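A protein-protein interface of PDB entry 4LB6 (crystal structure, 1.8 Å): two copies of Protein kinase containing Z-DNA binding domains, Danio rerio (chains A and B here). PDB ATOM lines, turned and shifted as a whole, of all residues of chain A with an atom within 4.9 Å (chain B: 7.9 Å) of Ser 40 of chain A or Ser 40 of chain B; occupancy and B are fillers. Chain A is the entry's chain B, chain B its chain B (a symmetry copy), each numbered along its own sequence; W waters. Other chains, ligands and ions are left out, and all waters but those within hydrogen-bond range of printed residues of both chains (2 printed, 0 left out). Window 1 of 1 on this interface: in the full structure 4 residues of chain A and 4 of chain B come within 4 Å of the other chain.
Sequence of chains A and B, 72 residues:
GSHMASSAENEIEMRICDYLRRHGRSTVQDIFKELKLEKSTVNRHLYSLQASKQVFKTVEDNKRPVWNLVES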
ATOM      1  N   GLU A  38       7.222 -19.203 -30.679  1.00  0.00           N
ATOM      2  CA  GLU A  38       6.235 -20.293 -30.778  1.00  0.00           C
ATOM      3  C   GLU A  38       6.447 -20.975 -32.123  1.00  0.00           C
ATOM      4  O   GLU A  38       6.707 -20.317 -33.117  1.00  0.00           O
ATOM      5  CB  GLU A  38       4.783 -19.727 -30.720  1.00  0.00           C
ATOM      6  CG  GLU A  38       4.393 -19.105 -29.350  1.00  0.00           C
ATOM      7  CD  GLU A  38       3.912 -20.161 -28.325  1.00  0.00           C
ATOM      8  OE1 GLU A  38       3.522 -21.287 -28.711  1.00  0.00           O
ATOM      9  OE2 GLU A  38       3.932 -19.874 -27.117  1.00  0.00           O
ATOM     10  N   LYS A  39       6.204 -22.260 -32.162  1.00  0.00           N
ATOM     11  CA  LYS A  39       6.233 -23.057 -33.403  1.00  0.00           C
ATOM     12  C   LYS A  39       5.265 -22.461 -34.411  1.00  0.00           C
ATOM     13  O   LYS A  39       5.635 -22.278 -35.570  1.00  0.00           O
ATOM     14  CB  LYS A  39       5.859 -24.505 -33.125  1.00  0.00           C
ATOM     15  CG  LYS A  39       5.845 -25.419 -34.382  1.00  0.00           C
ATOM     16  CD  LYS A  39       5.543 -26.896 -34.076  1.00  0.00           C
ATOM     17  CE  LYS A  39       4.078 -27.223 -33.823  1.00  0.00           C
ATOM     18  NZ  LYS A  39       3.343 -27.397 -35.156  1.00  0.00           N
ATOM     19  N   SER A  40       4.061 -22.092 -33.978  1.00  0.00           N
ATOM     20  CA  SER A  40       3.087 -21.577 -34.932  1.00  0.00           C
ATOM     21  C   SER A  40       3.583 -20.242 -35.544  1.00  0.00           C
ATOM     22  O   SER A  40       3.322 -19.953 -36.747  1.00  0.00           O
ATOM     23  CB  SER A  40       1.744 -21.384 -34.233  1.00  0.00           C
ATOM     24  OG  SER A  40       1.936 -20.427 -33.209  1.00  0.00           O
ATOM     25  N   THR A  41       4.277 -19.404 -34.753  1.00  0.00           N
ATOM     26  CA  THR A  41       4.796 -18.156 -35.310  1.00  0.00           C
ATOM     27  C   THR A  41       5.879 -18.449 -36.339  1.00  0.00           C
ATOM     28  O   THR A  41       5.963 -17.807 -37.379  1.00  0.00           O
ATOM     29  CB  THR A  41       5.412 -17.318 -34.187  1.00  0.00           C
ATOM     30  OG1 THR A  41       4.365 -17.034 -33.230  1.00  0.00           O
ATOM     31  CG2 THR A  41       6.059 -16.041 -34.738  1.00  0.00           C
ATOM     32  N   VAL A  42       6.771 -19.391 -36.042  1.00  0.00           N
ATOM     33  CA  VAL A  42       7.780 -19.688 -37.039  1.00  0.00           C
ATOM     34  C   VAL A  42       7.115 -20.300 -38.301  1.00  0.00           C
ATOM     35  O   VAL A  42       7.471 -19.943 -39.438  1.00  0.00           O
ATOM     36  CB  VAL A  42       8.854 -20.633 -36.454  1.00  0.00           C
ATOM     37  CG1 VAL A  42       9.859 -21.048 -37.521  1.00  0.00           C
ATOM     38  CG2 VAL A  42       9.573 -19.941 -35.260  1.00  0.00           C
ATOM     39  N   ASN A  43       6.171 -21.216 -38.118  1.00  0.00           N
ATOM     40  CA  ASN A  43       5.525 -21.769 -39.311  1.00  0.00           C
ATOM     41  C   ASN A  43       4.786 -20.693 -40.116  1.00  0.00           C
ATOM     42  O   ASN A  43       4.811 -20.756 -41.351  1.00  0.00           O
ATOM     43  CB  ASN A  43       4.542 -22.940 -38.994  1.00  0.00           C
ATOM     44  CG  ASN A  43       5.161 -24.296 -39.210  1.00  0.00           C
ATOM     45  OD1 ASN A  43       6.059 -24.470 -40.031  1.00  0.00           O
ATOM     46  ND2 ASN A  43       4.644 -25.312 -38.468  1.00  0.00           N
ATOM     47  N   ARG A  44       4.079 -19.764 -39.456  1.00  0.00           N
ATOM     48  CA  ARG A  44       3.358 -18.703 -40.199  1.00  0.00           C
ATOM     49  C   ARG A  44       4.371 -18.010 -41.122  1.00  0.00           C
ATOM     50  O   ARG A  44       4.111 -17.790 -42.336  1.00  0.00           O
ATOM     51  CB  ARG A  44       2.726 -17.661 -39.214  1.00  0.00           C
ATOM     52  CG  ARG A  44       2.176 -16.336 -39.809  1.00  0.00           C
ATOM     53  CD  ARG A  44       1.631 -15.435 -38.657  1.00  0.00           C
ATOM     54  NE  ARG A  44       0.895 -16.284 -37.728  1.00  0.00           N
ATOM     55  CZ  ARG A  44       1.117 -16.372 -36.416  1.00  0.00           C
ATOM     56  NH1 ARG A  44       1.993 -15.583 -35.825  1.00  0.00           N
ATOM     57  NH2 ARG A  44       0.429 -17.238 -35.688  1.00  0.00           N
ATOM     58  N   VAL B  28     -11.222 -22.160 -28.453  1.00  0.00           N
ATOM     59  CA  VAL B  28      -9.938 -21.458 -28.371  1.00  0.00           C
ATOM     60  C   VAL B  28      -9.925 -20.244 -29.324  1.00  0.00           C
ATOM     61  O   VAL B  28      -9.271 -19.230 -29.063  1.00  0.00           O
ATOM     62  CB  VAL B  28      -8.729 -22.400 -28.644  1.00  0.00           C
ATOM     63  CG1 VAL B  28      -8.762 -23.041 -30.101  1.00  0.00           C
ATOM     64  CG2 VAL B  28      -7.365 -21.679 -28.302  1.00  0.00           C
ATOM     65  N   PHE B  32      -8.463 -16.641 -28.128  1.00  0.00           N
ATOM     66  CA  PHE B  32      -7.190 -16.015 -28.576  1.00  0.00           C
ATOM     67  C   PHE B  32      -7.374 -14.700 -29.329  1.00  0.00           C
ATOM     68  O   PHE B  32      -6.510 -13.823 -29.295  1.00  0.00           O
ATOM     69  CB  PHE B  32      -6.245 -17.041 -29.329  1.00  0.00           C
ATOM     70  CG  PHE B  32      -6.444 -17.149 -30.837  1.00  0.00           C
ATOM     71  CD1 PHE B  32      -5.933 -16.209 -31.719  1.00  0.00           C
ATOM     72  CD2 PHE B  32      -7.084 -18.253 -31.370  1.00  0.00           C
ATOM     73  CE1 PHE B  32      -6.098 -16.323 -33.098  1.00  0.00           C
ATOM     74  CE2 PHE B  32      -7.277 -18.371 -32.744  1.00  0.00           C
ATOM     75  CZ  PHE B  32      -6.785 -17.409 -33.629  1.00  0.00           C
ATOM     76  N   LEU B  37      -3.541 -13.326 -28.145  1.00  0.00           N
ATOM     77  CA  LEU B  37      -2.454 -14.266 -27.877  1.00  0.00           C
ATOM     78  C   LEU B  37      -2.406 -15.284 -29.057  1.00  0.00           C
ATOM     79  O   LEU B  37      -3.330 -15.339 -29.865  1.00  0.00           O
ATOM     80  CB  LEU B  37      -2.710 -15.038 -26.592  1.00  0.00           C
ATOM     81  CG  LEU B  37      -2.839 -14.104 -25.356  1.00  0.00           C
ATOM     82  CD1 LEU B  37      -3.520 -14.939 -24.242  1.00  0.00           C
ATOM     83  CD2 LEU B  37      -1.458 -13.602 -24.943  1.00  0.00           C
ATOM     84  N   GLU B  38      -1.333 -16.066 -29.175  1.00  0.00           N
ATOM     85  CA  GLU B  38      -1.333 -17.133 -30.192  1.00  0.00           C
ATOM     86  C   GLU B  38      -2.339 -18.185 -29.744  1.00  0.00           C
ATOM     87  O   GLU B  38      -2.436 -18.487 -28.567  1.00  0.00           O
ATOM     88  CB  GLU B  38       0.077 -17.791 -30.298  1.00  0.00           C
ATOM     89  CG  GLU B  38       1.181 -16.853 -30.861  1.00  0.00           C
ATOM     90  CD  GLU B  38       1.199 -16.807 -32.408  1.00  0.00           C
ATOM     91  OE1 GLU B  38       0.658 -17.718 -33.076  1.00  0.00           O
ATOM     92  OE2 GLU B  38       1.750 -15.847 -32.971  1.00  0.00           O
ATOM     93  N   LYS B  39      -2.974 -18.818 -30.698  1.00  0.00           N
ATOM     94  CA  LYS B  39      -3.886 -19.952 -30.455  1.00  0.00           C
ATOM     95  C   LYS B  39      -3.146 -21.047 -29.705  1.00  0.00           C
ATOM     96  O   LYS B  39      -3.669 -21.565 -28.720  1.00  0.00           O
ATOM     97  CB  LYS B  39      -4.425 -20.501 -31.767  1.00  0.00           C
ATOM     98  CG  LYS B  39      -5.385 -21.714 -31.611  1.00  0.00           C
ATOM     99  CD  LYS B  39      -5.985 -22.209 -32.937  1.00  0.00           C
ATOM    100  CE  LYS B  39      -5.057 -23.056 -33.797  1.00  0.00           C
ATOM    101  NZ  LYS B  39      -5.067 -24.506 -33.304  1.00  0.00           N
ATOM    102  N   SER B  40      -1.916 -21.359 -30.109  1.00  0.00           N
ATOM    103  CA  SER B  40      -1.205 -22.448 -29.452  1.00  0.00           C
ATOM    104  C   SER B  40      -0.929 -22.097 -27.968  1.00  0.00           C
ATOM    105  O   SER B  40      -0.949 -22.999 -27.082  1.00  0.00           O
ATOM    106  CB  SER B  40       0.101 -22.722 -30.193  1.00  0.00           C
ATOM    107  OG  SER B  40       0.884 -21.547 -30.115  1.00  0.00           O
ATOM    108  N   THR B  41      -0.653 -20.816 -27.663  1.00  0.00           N
ATOM    109  CA  THR B  41      -0.432 -20.443 -26.267  1.00  0.00           C
ATOM    110  C   THR B  41      -1.718 -20.596 -25.469  1.00  0.00           C
ATOM    111  O   THR B  41      -1.715 -21.046 -24.329  1.00  0.00           O
ATOM    112  CB  THR B  41       0.007 -18.978 -26.198  1.00  0.00           C
ATOM    113  OG1 THR B  41       1.240 -18.856 -26.945  1.00  0.00           O
ATOM    114  CG2 THR B  41       0.158 -18.511 -24.745  1.00  0.00           C
ATOM    115  N   VAL B  42      -2.846 -20.169 -26.032  1.00  0.00           N
ATOM    116  CA  VAL B  42      -4.073 -20.348 -25.281  1.00  0.00           C
ATOM    117  C   VAL B  42      -4.379 -21.860 -25.119  1.00  0.00           C
ATOM    118  O   VAL B  42      -4.778 -22.309 -24.029  1.00  0.00           O
ATOM    119  CB  VAL B  42      -5.240 -19.606 -25.972  1.00  0.00           C
ATOM    120  CG1 VAL B  42      -6.559 -19.878 -25.261  1.00  0.00           C
ATOM    121  CG2 VAL B  42      -4.943 -18.079 -26.018  1.00  0.00           C
ATOM    122  N   ASN B  43      -4.212 -22.641 -26.179  1.00  0.00           N
ATOM    123  CA  ASN B  43      -4.475 -24.074 -26.014  1.00  0.00           C
ATOM    124  C   ASN B  43      -3.536 -24.714 -24.984  1.00  0.00           C
ATOM    125  O   ASN B  43      -3.990 -25.586 -24.232  1.00  0.00           O
ATOM    126  CB  ASN B  43      -4.394 -24.875 -27.351  1.00  0.00           C
ATOM    127  CG  ASN B  43      -5.747 -25.122 -27.964  1.00  0.00           C
ATOM    128  OD1 ASN B  43      -6.762 -25.203 -27.275  1.00  0.00           O
ATOM    129  ND2 ASN B  43      -5.768 -25.283 -29.315  1.00  0.00           N
ATOM    130  N   ARG B  44      -2.243 -24.361 -24.980  1.00  0.00           N
ATOM    131  CA  ARG B  44      -1.307 -24.953 -23.994  1.00  0.00           C
ATOM    132  C   ARG B  44      -1.899 -24.726 -22.595  1.00  0.00           C
ATOM    133  O   ARG B  44      -1.965 -25.660 -21.751  1.00  0.00           O
ATOM    134  CB  ARG B  44       0.107 -24.286 -24.095  1.00  0.00           C
ATOM    135  CG  ARG B  44       1.131 -24.574 -22.963  1.00  0.00           C
ATOM    136  CD  ARG B  44       2.450 -23.786 -23.241  1.00  0.00           C
ATOM    137  NE  ARG B  44       2.749 -23.891 -24.664  1.00  0.00           N
ATOM    138  CZ  ARG B  44       2.956 -22.866 -25.491  1.00  0.00           C
ATOM    139  NH1 ARG B  44       3.006 -21.630 -25.034  1.00  0.00           N
ATOM    140  NH2 ARG B  44       3.146 -23.089 -26.783  1.00  0.00           N
ATOM    141  N   HIS B  45      -2.315 -23.487 -22.352  1.00  0.00           N
ATOM    142  CA  HIS B  45      -2.854 -23.168 -21.017  1.00  0.00           C
ATOM    143  C   HIS B  45      -4.212 -23.792 -20.731  1.00  0.00           C
ATOM    144  O   HIS B  45      -4.469 -24.142 -19.583  1.00  0.00           O
ATOM    145  CB  HIS B  45      -2.824 -21.645 -20.777  1.00  0.00           C
ATOM    146  CG  HIS B  45      -1.428 -21.136 -20.586  1.00  0.00           C
ATOM    147  ND1 HIS B  45      -0.706 -21.362 -19.425  1.00  0.00           N
ATOM    148  CD2 HIS B  45      -0.593 -20.486 -21.427  1.00  0.00           C
ATOM    149  CE1 HIS B  45       0.497 -20.826 -19.549  1.00  0.00           C
ATOM    150  NE2 HIS B  45       0.589 -20.282 -20.752  1.00  0.00           N
ATOM    151  N   LEU B  46      -5.088 -23.923 -21.742  1.00  0.00           N
ATOM    152  CA  LEU B  46      -6.378 -24.580 -21.502  1.00  0.00           C
ATOM    153  C   LEU B  46      -6.169 -26.035 -21.082  1.00  0.00           C
ATOM    154  O   LEU B  46      -6.798 -26.520 -20.111  1.00  0.00           O
ATOM    155  CB  LEU B  46      -7.219 -24.560 -22.795  1.00  0.00           C
ATOM    156  CG  LEU B  46      -7.912 -23.204 -23.005  1.00  0.00           C
ATOM    157  CD1 LEU B  46      -8.491 -23.161 -24.454  1.00  0.00           C
ATOM    158  CD2 LEU B  46      -9.038 -22.967 -22.026  1.00  0.00           C
ATOM    159  N   TYR B  47      -5.277 -26.726 -21.800  1.00  0.00           N
ATOM    160  CA  TYR B  47      -5.005 -28.150 -21.481  1.00  0.00           C
ATOM    161  C   TYR B  47      -4.385 -28.261 -20.095  1.00  0.00           C
ATOM    162  O   TYR B  47      -4.760 -29.139 -19.285  1.00  0.00           O
ATOM    163  CB  TYR B  47      -4.164 -28.866 -22.569  1.00  0.00           C
ATOM    164  CG  TYR B  47      -5.068 -29.275 -23.723  1.00  0.00           C
ATOM    165  CD1 TYR B  47      -5.300 -28.402 -24.806  1.00  0.00           C
ATOM    166  CD2 TYR B  47      -5.815 -30.468 -23.654  1.00  0.00           C
ATOM    167  CE1 TYR B  47      -6.188 -28.755 -25.837  1.00  0.00           C
ATOM    168  CE2 TYR B  47      -6.692 -30.841 -24.677  1.00  0.00           C
ATOM    169  CZ  TYR B  47      -6.909 -29.979 -25.754  1.00  0.00           C
ATOM    170  OH  TYR B  47      -7.767 -30.382 -26.780  1.00  0.00           O
HETATM  171  O   HOH W   1      -0.848 -20.559 -32.689  1.00  0.00           O
HETATM  172  O   HOH W   2       2.964 -22.955 -31.431  1.00  0.00           O
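OE1 of Glu 38 of chain A lies within hydrogen-bond range of OG of Ser 40 of chain B (3.0 Å).
The guanidinium group (NH2) of Arg 44 of chain A lies within salt-bridge range of the side-chain carboxylate (OE1) of Glu 38 of chain B, at 2.7 Å.
OG of Ser 40 of chain B lies within hydrogen-bond range of OG of Ser 40 of chain A, at 3.5 Å.
The side-chain hydroxyl (OG) of Ser 40 of chain A sits at hydrogen-bond distance from the side-chain carboxylate (OE1) of Glu 38 of chain B (3.0 Å).
The side-chain hydroxyl of Thr 41 of chain A lies within hydrogen-bond range of the side-chain carboxylate of Glu 38 of chain B (2.9 Å).
The guanidinium group (NH2) of Arg 44 of chain B is in salt-bridge range of the side-chain carboxylate (OE1) of Glu 38 of chain A (2.7 Å).
The side-chain hydroxyl (OG1) of Thr 41 of chain B lies within hydrogen-bond range of the side-chain carboxylate (OE2) of Glu 38 of chain A.
Printed residues of chain B within 4 Å of Ser 40 of chain A: Glu 38 (3.0 Å) and Ser 40 (3.5 Å).
Of the printed residues of chain A, Ser 40 of chain B touches Glu 38 (3.0 Å) and Ser 40 (3.5 Å).
Of the printed residues of chain B, Glu 38 of chain A touches Ser 40 (3.0 Å), Thr 41 (2.9 Å) and Arg 44 (2.7 Å).
Of the printed residues of chain A, Glu 38 of chain B touches Ser 40, Thr 41 and Arg 44.
Printed residues of chain A within 4 Å of Arg 44 of chain B: Glu 38 (2.7 Å).
Printed residues of chain B within 4 Å of Thr 41 of chain A: Glu 38.
Printed residues of chain A within 4 Å of Thr 41 of chain B: Glu 38.
His 45 of chain B touches none of the printed residues of chain A.
Val 28 of chain B touches none of the printed residues of chain A.
The nearest printed residue of chain A that does not touch Ser 40 of chain B is Lys 39 of chain A (5.7 Å).
The nearest printed residue of chain B that does not touch Arg 44 of chain A is Lys 39 of chain B (6.2 Å).
Of the 7 printed residues of chain A, 4 touch a printed residue of chain B.
Among the printed residues, 7 pairs touch across the chains.
Glu 38 of chain A touches Ser 40 of chain B, and with the chains exchanged Ser 40 of chain A touches Glu 38 of chain B.
Glu 38 of chain A touches Thr 41 of chain B, and with the chains exchanged Thr 41 of chain A touches Glu 38 of chain B.
Glu 38 of chain A touches Arg 44 of chain B, and with the chains exchanged Arg 44 of chain A touches Glu 38 of chain B.
Ser 40 of chain B touches its own counterpart, Ser 40 of chain A.
Positions printed for both chains: 38, 39, 40, 41, 42, 43 and 44.
Of the 7 pairs that touch across the chains among the printed residues, 7 have their exchanged pair printed and touching as well.
Water W1 lies within hydrogen-bond range of OG of Ser 40 of chain A (2.8 Å), N of Ser 40 of chain B (2.9 Å), OE1 of Glu 38 of chain B (3.2 Å) and N of Lys 39 of chain B (3.4 Å).
Water W2 lies within hydrogen-bond range of the side-chain hydroxyl of Ser 40 of chain B (2.8 Å), the backbone NH of Ser 40 of chain A (2.9 Å), the side-chain carboxylate of Glu 38 of chain A (3.2 Å) and the backbone NH of Lys 39 of chain A (3.4 Å).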
